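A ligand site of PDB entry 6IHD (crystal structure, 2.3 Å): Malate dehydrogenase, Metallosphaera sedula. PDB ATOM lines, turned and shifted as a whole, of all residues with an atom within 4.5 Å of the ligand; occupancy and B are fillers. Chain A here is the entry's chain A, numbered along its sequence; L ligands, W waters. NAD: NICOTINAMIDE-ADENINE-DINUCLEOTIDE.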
ATOM      1  N   ILE A   6       4.605   1.996  -5.694  1.00  0.00           N
ATOM      2  CA  ILE A   6       4.986   3.148  -6.488  1.00  0.00           C
ATOM      3  C   ILE A   6       6.506   3.206  -6.509  1.00  0.00           C
ATOM      4  O   ILE A   6       7.192   3.689  -5.566  1.00  0.00           O
ATOM      5  CB  ILE A   6       4.407   4.496  -5.970  1.00  0.00           C
ATOM      6  CG1 ILE A   6       2.905   4.400  -5.649  1.00  0.00           C
ATOM      7  CG2 ILE A   6       4.602   5.593  -7.006  1.00  0.00           C
ATOM      8  CD1 ILE A   6       2.056   3.789  -6.741  1.00  0.00           C
ATOM      9  N   GLY A   7       7.021   2.716  -7.632  1.00  0.00           N
ATOM     10  CA  GLY A   7       8.427   2.572  -7.809  1.00  0.00           C
ATOM     11  C   GLY A   7       8.772   1.111  -7.776  1.00  0.00           C
ATOM     12  O   GLY A   7       8.505   0.445  -6.791  1.00  0.00           O
ATOM     13  N   ALA A   8       9.337   0.669  -8.879  1.00  0.00           N
ATOM     14  CA  ALA A   8       9.695  -0.686  -9.172  1.00  0.00           C
ATOM     15  C   ALA A   8      11.187  -0.744  -9.546  1.00  0.00           C
ATOM     16  O   ALA A   8      11.536  -1.442 -10.498  1.00  0.00           O
ATOM     17  CB  ALA A   8       8.874  -1.191 -10.365  1.00  0.00           C
ATOM     18  N   GLY A   9      12.049   0.037  -8.872  1.00  0.00           N
ATOM     19  CA  GLY A   9      13.500  -0.147  -8.986  1.00  0.00           C
ATOM     20  C   GLY A   9      14.023  -1.118  -7.921  1.00  0.00           C
ATOM     21  O   GLY A   9      13.263  -1.812  -7.258  1.00  0.00           O
ATOM     22  N   LYS A  10      15.328  -1.110  -7.731  1.00  0.00           N
ATOM     23  CA  LYS A  10      16.017  -1.980  -6.770  1.00  0.00           C
ATOM     24  C   LYS A  10      15.277  -2.215  -5.436  1.00  0.00           C
ATOM     25  O   LYS A  10      14.898  -3.352  -5.155  1.00  0.00           O
ATOM     26  CB  LYS A  10      17.405  -1.408  -6.501  1.00  0.00           C
ATOM     27  CG  LYS A  10      18.397  -1.712  -7.657  1.00  0.00           C
ATOM     28  CD  LYS A  10      19.713  -0.922  -7.532  1.00  0.00           C
ATOM     29  CE  LYS A  10      19.480   0.594  -7.376  1.00  0.00           C
ATOM     30  NZ  LYS A  10      20.306   1.489  -8.238  1.00  0.00           N
ATOM     31  N   ILE A  11      15.086  -1.173  -4.615  1.00  0.00           N
ATOM     32  CA  ILE A  11      14.386  -1.358  -3.339  1.00  0.00           C
ATOM     33  C   ILE A  11      12.891  -1.717  -3.522  1.00  0.00           C
ATOM     34  O   ILE A  11      12.397  -2.563  -2.787  1.00  0.00           O
ATOM     35  CB  ILE A  11      14.561  -0.171  -2.366  1.00  0.00           C
ATOM     36  CG1 ILE A  11      14.329  -0.614  -0.922  1.00  0.00           C
ATOM     37  CG2 ILE A  11      13.629   0.989  -2.648  1.00  0.00           C
ATOM     38  CD1 ILE A  11      15.234  -1.754  -0.496  1.00  0.00           C
ATOM     39  N   GLY A  12      12.192  -1.118  -4.504  1.00  0.00           N
ATOM     40  CA  GLY A  12      10.784  -1.487  -4.725  1.00  0.00           C
ATOM     41  C   GLY A  12      10.557  -2.936  -5.165  1.00  0.00           C
ATOM     42  O   GLY A  12       9.683  -3.625  -4.665  1.00  0.00           O
ATOM     43  N   TYR A  31       3.891  -0.031 -10.176  1.00  0.00           N
ATOM     44  CA  TYR A  31       3.936   1.089 -11.082  1.00  0.00           C
ATOM     45  C   TYR A  31       5.281   1.741 -11.045  1.00  0.00           C
ATOM     46  O   TYR A  31       5.856   1.939 -10.008  1.00  0.00           O
ATOM     47  CB  TYR A  31       2.857   2.150 -10.709  1.00  0.00           C
ATOM     48  CG  TYR A  31       3.022   3.478 -11.455  1.00  0.00           C
ATOM     49  CD1 TYR A  31       2.614   3.621 -12.787  1.00  0.00           C
ATOM     50  CD2 TYR A  31       3.647   4.569 -10.853  1.00  0.00           C
ATOM     51  CE1 TYR A  31       2.812   4.807 -13.489  1.00  0.00           C
ATOM     52  CE2 TYR A  31       3.799   5.779 -11.525  1.00  0.00           C
ATOM     53  CZ  TYR A  31       3.398   5.889 -12.820  1.00  0.00           C
ATOM     54  OH  TYR A  31       3.597   7.081 -13.463  1.00  0.00           O
ATOM     55  N   ASP A  32       5.716   2.146 -12.224  1.00  0.00           N
ATOM     56  CA  ASP A  32       6.964   2.898 -12.417  1.00  0.00           C
ATOM     57  C   ASP A  32       6.772   3.741 -13.670  1.00  0.00           C
ATOM     58  O   ASP A  32       5.976   3.408 -14.541  1.00  0.00           O
ATOM     59  CB  ASP A  32       8.163   1.936 -12.563  1.00  0.00           C
ATOM     60  CG  ASP A  32       9.519   2.619 -12.230  1.00  0.00           C
ATOM     61  OD1 ASP A  32      10.017   3.413 -13.119  1.00  0.00           O
ATOM     62  OD2 ASP A  32      10.066   2.381 -11.089  1.00  0.00           O
ATOM     63  N   ILE A  33       7.488   4.843 -13.763  1.00  0.00           N
ATOM     64  CA  ILE A  33       7.481   5.618 -15.018  1.00  0.00           C
ATOM     65  C   ILE A  33       8.325   4.977 -16.133  1.00  0.00           C
ATOM     66  O   ILE A  33       8.044   5.287 -17.301  1.00  0.00           O
ATOM     67  CB  ILE A  33       7.936   7.069 -14.807  1.00  0.00           C
ATOM     68  CG1 ILE A  33       9.438   7.111 -14.380  1.00  0.00           C
ATOM     69  CG2 ILE A  33       7.046   7.757 -13.761  1.00  0.00           C
ATOM     70  CD1 ILE A  33       9.995   8.484 -14.110  1.00  0.00           C
ATOM     71  N   ILE A  34       9.316   4.102 -15.827  1.00  0.00           N
ATOM     72  CA  ILE A  34      10.174   3.511 -16.901  1.00  0.00           C
ATOM     73  C   ILE A  34       9.347   2.575 -17.758  1.00  0.00           C
ATOM     74  O   ILE A  34       8.720   1.704 -17.250  1.00  0.00           O
ATOM     75  CB  ILE A  34      11.401   2.710 -16.426  1.00  0.00           C
ATOM     76  CG1 ILE A  34      12.394   3.686 -15.766  1.00  0.00           C
ATOM     77  CG2 ILE A  34      12.049   1.945 -17.627  1.00  0.00           C
ATOM     78  CD1 ILE A  34      13.396   3.077 -14.809  1.00  0.00           C
ATOM     79  N   LEU A  37       9.044  -1.671 -17.609  1.00  0.00           N
ATOM     80  CA  LEU A  37       9.694  -2.286 -16.470  1.00  0.00           C
ATOM     81  C   LEU A  37       8.664  -3.077 -15.585  1.00  0.00           C
ATOM     82  O   LEU A  37       8.892  -4.240 -15.307  1.00  0.00           O
ATOM     83  CB  LEU A  37      10.376  -1.233 -15.670  1.00  0.00           C
ATOM     84  CG  LEU A  37      10.936  -1.578 -14.302  1.00  0.00           C
ATOM     85  CD1 LEU A  37      12.117  -2.490 -14.495  1.00  0.00           C
ATOM     86  CD2 LEU A  37      11.464  -0.296 -13.661  1.00  0.00           C
ATOM     87  N   SER A  76       8.391   4.028  -3.191  1.00  0.00           N
ATOM     88  CA  SER A  76       9.867   3.997  -3.269  1.00  0.00           C
ATOM     89  C   SER A  76      10.395   4.796  -4.496  1.00  0.00           C
ATOM     90  O   SER A  76      11.557   4.694  -4.886  1.00  0.00           O
ATOM     91  CB  SER A  76      10.347   2.529  -3.280  1.00  0.00           C
ATOM     92  OG  SER A  76       9.888   1.895  -4.453  1.00  0.00           O
ATOM     93  N   ALA A  77       9.536   5.600  -5.105  1.00  0.00           N
ATOM     94  CA  ALA A  77       9.941   6.430  -6.227  1.00  0.00           C
ATOM     95  C   ALA A  77      10.835   7.568  -5.729  1.00  0.00           C
ATOM     96  O   ALA A  77      10.484   8.273  -4.785  1.00  0.00           O
ATOM     97  CB  ALA A  77       8.722   6.969  -6.962  1.00  0.00           C
ATOM     98  N   GLY A  78      11.994   7.717  -6.383  1.00  0.00           N
ATOM     99  CA  GLY A  78      13.088   8.535  -5.882  1.00  0.00           C
ATOM    100  C   GLY A  78      14.058   8.889  -6.993  1.00  0.00           C
ATOM    101  O   GLY A  78      14.096   8.230  -8.039  1.00  0.00           O
ATOM    102  N   ILE A  97       7.932  14.749  -6.361  1.00  0.00           N
ATOM    103  CA  ILE A  97       7.342  13.470  -6.677  1.00  0.00           C
ATOM    104  C   ILE A  97       6.167  13.228  -5.711  1.00  0.00           C
ATOM    105  O   ILE A  97       5.088  12.829  -6.142  1.00  0.00           O
ATOM    106  CB  ILE A  97       8.340  12.308  -6.571  1.00  0.00           C
ATOM    107  CG1 ILE A  97       9.425  12.388  -7.649  1.00  0.00           C
ATOM    108  CG2 ILE A  97       7.639  10.960  -6.725  1.00  0.00           C
ATOM    109  CD1 ILE A  97      10.647  11.553  -7.296  1.00  0.00           C
ATOM    110  N   VAL A 117       9.143   4.815   1.698  1.00  0.00           N
ATOM    111  CA  VAL A 117      10.469   4.245   1.617  1.00  0.00           C
ATOM    112  C   VAL A 117      11.473   5.236   0.995  1.00  0.00           C
ATOM    113  O   VAL A 117      12.648   5.298   1.421  1.00  0.00           O
ATOM    114  CB  VAL A 117      10.410   2.917   0.794  1.00  0.00           C
ATOM    115  CG1 VAL A 117      11.810   2.280   0.641  1.00  0.00           C
ATOM    116  CG2 VAL A 117       9.382   1.977   1.399  1.00  0.00           C
ATOM    117  N   ALA A 118      11.043   5.974  -0.023  1.00  0.00           N
ATOM    118  CA  ALA A 118      11.949   6.943  -0.700  1.00  0.00           C
ATOM    119  C   ALA A 118      12.537   7.951   0.294  1.00  0.00           C
ATOM    120  O   ALA A 118      11.876   8.342   1.249  1.00  0.00           O
ATOM    121  CB  ALA A 118      11.210   7.662  -1.798  1.00  0.00           C
ATOM    122  N   ASN A 119      13.796   8.311   0.090  1.00  0.00           N
ATOM    123  CA  ASN A 119      14.518   9.198   1.005  1.00  0.00           C
ATOM    124  C   ASN A 119      14.418  10.669   0.598  1.00  0.00           C
ATOM    125  O   ASN A 119      14.175  10.927  -0.570  1.00  0.00           O
ATOM    126  CB  ASN A 119      16.011   8.812   1.055  1.00  0.00           C
ATOM    127  CG  ASN A 119      16.288   7.770   2.118  1.00  0.00           C
ATOM    128  OD1 ASN A 119      15.741   7.824   3.239  1.00  0.00           O
ATOM    129  ND2 ASN A 119      17.116   6.792   1.772  1.00  0.00           N
ATOM    130  N   VAL A 121      13.469   9.802   4.147  1.00  0.00           N
ATOM    131  CA  VAL A 121      12.261   8.992   4.348  1.00  0.00           C
ATOM    132  C   VAL A 121      11.279   9.617   5.342  1.00  0.00           C
ATOM    133  O   VAL A 121      10.102   9.716   5.046  1.00  0.00           O
ATOM    134  CB  VAL A 121      12.603   7.475   4.643  1.00  0.00           C
ATOM    135  CG1 VAL A 121      13.328   7.286   5.982  1.00  0.00           C
ATOM    136  CG2 VAL A 121      11.356   6.593   4.599  1.00  0.00           C
ATOM    137  N   ALA A 139       9.172   3.883   7.039  1.00  0.00           N
ATOM    138  CA  ALA A 139      10.095   2.793   7.412  1.00  0.00           C
ATOM    139  C   ALA A 139      11.055   3.148   8.539  1.00  0.00           C
ATOM    140  O   ALA A 139      11.471   2.279   9.297  1.00  0.00           O
ATOM    141  CB  ALA A 139      10.904   2.372   6.187  1.00  0.00           C
ATOM    142  N   VAL A 143      15.255  -0.383   9.815  1.00  0.00           N
ATOM    143  CA  VAL A 143      16.438  -0.981   9.172  1.00  0.00           C
ATOM    144  C   VAL A 143      17.634  -0.897  10.137  1.00  0.00           C
ATOM    145  O   VAL A 143      18.240  -1.903  10.495  1.00  0.00           O
ATOM    146  CB  VAL A 143      16.721  -0.313   7.848  1.00  0.00           C
ATOM    147  CG1 VAL A 143      18.049  -0.795   7.239  1.00  0.00           C
ATOM    148  CG2 VAL A 143      15.561  -0.559   6.908  1.00  0.00           C
ATOM    149  N   THR A 217      21.757  -0.616  -1.359  1.00  0.00           N
ATOM    150  CA  THR A 217      21.285  -1.603  -0.498  1.00  0.00           C
ATOM    151  C   THR A 217      19.948  -2.102  -1.008  1.00  0.00           C
ATOM    152  O   THR A 217      19.099  -1.308  -1.373  1.00  0.00           O
ATOM    153  CB  THR A 217      21.036  -0.949   0.867  1.00  0.00           C
ATOM    154  OG1 THR A 217      20.033   0.069   0.730  1.00  0.00           O
ATOM    155  CG2 THR A 217      22.310  -0.324   1.420  1.00  0.00           C
ATOM    156  N   PRO A 221      17.286  -3.910   3.692  1.00  0.00           N
ATOM    157  CA  PRO A 221      16.068  -3.080   3.874  1.00  0.00           C
ATOM    158  C   PRO A 221      14.830  -3.580   3.116  1.00  0.00           C
ATOM    159  O   PRO A 221      13.687  -3.440   3.603  1.00  0.00           O
ATOM    160  CB  PRO A 221      16.483  -1.690   3.406  1.00  0.00           C
ATOM    161  CG  PRO A 221      17.779  -1.838   2.720  1.00  0.00           C
ATOM    162  CD  PRO A 221      18.418  -3.142   3.145  1.00  0.00           C
ATOM    163  N   ILE A 225      11.603  -4.083   5.531  1.00  0.00           N
ATOM    164  CA  ILE A 225      10.451  -3.272   5.226  1.00  0.00           C
ATOM    165  C   ILE A 225       9.290  -4.183   4.817  1.00  0.00           C
ATOM    166  O   ILE A 225       8.173  -3.924   5.230  1.00  0.00           O
ATOM    167  CB  ILE A 225      10.774  -2.215   4.158  1.00  0.00           C
ATOM    168  CG1 ILE A 225      11.739  -1.183   4.711  1.00  0.00           C
ATOM    169  CG2 ILE A 225       9.528  -1.456   3.770  1.00  0.00           C
ATOM    170  CD1 ILE A 225      12.291  -0.228   3.697  1.00  0.00           C
HETATM  171  PA  NAD L   1      16.241   3.123  -8.169  1.00  0.00           P
HETATM  172  O1A NAD L   1      16.748   4.318  -8.841  1.00  0.00           O
HETATM  173  O2A NAD L   1      16.700   1.814  -8.643  1.00  0.00           O
HETATM  174  O5B NAD L   1      14.678   3.144  -8.178  1.00  0.00           O
HETATM  175  C5B NAD L   1      13.901   4.296  -8.375  1.00  0.00           C
HETATM  176  C4B NAD L   1      12.751   3.924  -9.280  1.00  0.00           C
HETATM  177  O4B NAD L   1      11.667   4.809  -9.116  1.00  0.00           O
HETATM  178  C3B NAD L   1      13.103   4.008 -10.754  1.00  0.00           C
HETATM  179  O3B NAD L   1      12.679   2.795 -11.327  1.00  0.00           O
HETATM  180  C2B NAD L   1      12.279   5.153 -11.298  1.00  0.00           C
HETATM  181  O2B NAD L   1      11.840   4.948 -12.622  1.00  0.00           O
HETATM  182  C1B NAD L   1      11.118   5.113 -10.373  1.00  0.00           C
HETATM  183  N9A NAD L   1      10.532   6.451 -10.321  1.00  0.00           N
HETATM  184  C8A NAD L   1      11.144   7.631 -10.272  1.00  0.00           C
HETATM  185  N7A NAD L   1      10.260   8.623 -10.225  1.00  0.00           N
HETATM  186  C5A NAD L   1       9.050   8.064 -10.248  1.00  0.00           C
HETATM  187  C6A NAD L   1       7.665   8.512 -10.223  1.00  0.00           C
HETATM  188  N6A NAD L   1       7.311   9.796 -10.168  1.00  0.00           N
HETATM  189  N1A NAD L   1       6.717   7.609 -10.248  1.00  0.00           N
HETATM  190  C2A NAD L   1       7.001   6.313 -10.300  1.00  0.00           C
HETATM  191  N3A NAD L   1       8.229   5.821 -10.333  1.00  0.00           N
HETATM  192  C4A NAD L   1       9.256   6.642 -10.301  1.00  0.00           C
HETATM  193  O3  NAD L   1      16.642   3.336  -6.670  1.00  0.00           O
HETATM  194  PN  NAD L   1      16.276   2.434  -5.430  1.00  0.00           P
HETATM  195  O1N NAD L   1      17.518   1.839  -4.937  1.00  0.00           O
HETATM  196  O2N NAD L   1      15.097   1.607  -5.734  1.00  0.00           O
HETATM  197  O5D NAD L   1      15.855   3.482  -4.345  1.00  0.00           O
HETATM  198  C5D NAD L   1      14.611   4.130  -4.400  1.00  0.00           C
HETATM  199  C4D NAD L   1      14.475   5.157  -3.279  1.00  0.00           C
HETATM  200  O4D NAD L   1      14.283   4.535  -2.013  1.00  0.00           O
HETATM  201  C3D NAD L   1      15.721   5.978  -3.168  1.00  0.00           C
HETATM  202  O3D NAD L   1      15.310   7.274  -2.809  1.00  0.00           O
HETATM  203  C2D NAD L   1      16.427   5.370  -2.006  1.00  0.00           C
HETATM  204  O2D NAD L   1      17.221   6.335  -1.345  1.00  0.00           O
HETATM  205  C1D NAD L   1      15.299   4.892  -1.123  1.00  0.00           C
HETATM  206  N1N NAD L   1      15.709   3.790  -0.247  1.00  0.00           N
HETATM  207  C2N NAD L   1      15.289   3.763   0.994  1.00  0.00           C
HETATM  208  C3N NAD L   1      15.647   2.754   1.854  1.00  0.00           C
HETATM  209  C7N NAD L   1      15.168   2.722   3.250  1.00  0.00           C
HETATM  210  O7N NAD L   1      14.197   3.320   3.557  1.00  0.00           O
HETATM  211  N7N NAD L   1      15.846   2.024   4.136  1.00  0.00           N
HETATM  212  C4N NAD L   1      16.470   1.750   1.419  1.00  0.00           C
HETATM  213  C5N NAD L   1      16.899   1.798   0.114  1.00  0.00           C
HETATM  214  C6N NAD L   1      16.510   2.831  -0.693  1.00  0.00           C
HETATM  215  O   HOH W   1      12.268   1.402  -6.120  1.00  0.00           O
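O of Val 117 sits close to O7N of the ligand (3.3 Å).
Gly 9 touches the ligand.
Tyr 31 touches the ligand (CE2 to C2A, 3.5 Å).
Ile 33 touches the ligand (CG2 to N1A, 3.5 Å).
Ile 34 touches the ligand.
Ser 76 touches the ligand (O to C5D, 3.1 Å).
Ala 77 touches the ligand.
O of Gly 78 touches C8A of the ligand, 3.7 Å away.
Ile 97 touches the ligand.
Ala 118 touches the ligand.
Val 143 touches the ligand.
Thr 217 touches the ligand.
CB of Pro 221 touches N7N of the ligand, 3.8 Å away.
Of the 25 residues printed, 17 come within 4 Å of the ligand.
The nearest printed residue that does not touch the ligand is Ile 225 (4.03 Å).
Water W1 lies within hydrogen-bond range of O2N of the ligand, OG of Ser 76, N of Gly 12 and N of Gly 9.
OD1 of Asp 32 sits at hydrogen-bond distance from O2B of the ligand.
N of Ile 11 is in hydrogen-bond range of O2N of the ligand.
The backbone NH of Lys 10 sits close to an oxygen (O2A) of the ligand (3.4 Å).
The side-chain amino group (NZ) of Lys 10 is in salt-bridge range of an oxygen (O2A) of the ligand, 3.6 Å away.
O3D of the ligand sits at hydrogen-bond distance from N of Asn 119 (3.4 Å).
ND2 of Asn 119 is in hydrogen-bond range of O2D of the ligand (3.2 Å).
N of Ser 76 lies within hydrogen-bond range of O of Ile 6 (2.7 Å).
The backbone NH (N) of Gly 7 sits at hydrogen-bond distance from the backbone carbonyl oxygen (O) of Tyr 31, at 2.8 Å.
The side-chain hydroxyl (OG) of Ser 76 is in hydrogen-bond range of the backbone carbonyl oxygen (O) of Gly 7 (3.1 Å).
N of Ala 77 lies within hydrogen-bond range of O of Ile 6, 3.1 Å away.
OD1 of Asn 119 lies within hydrogen-bond range of N of Val 121 (3.1 Å).
The backbone NH (N) of Ile 34 sits at hydrogen-bond distance from the side-chain carboxylate (OD1) of Asp 32, 2.9 Å away.
OD2 of Asp 32 is in hydrogen-bond range of N of Ala 8.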
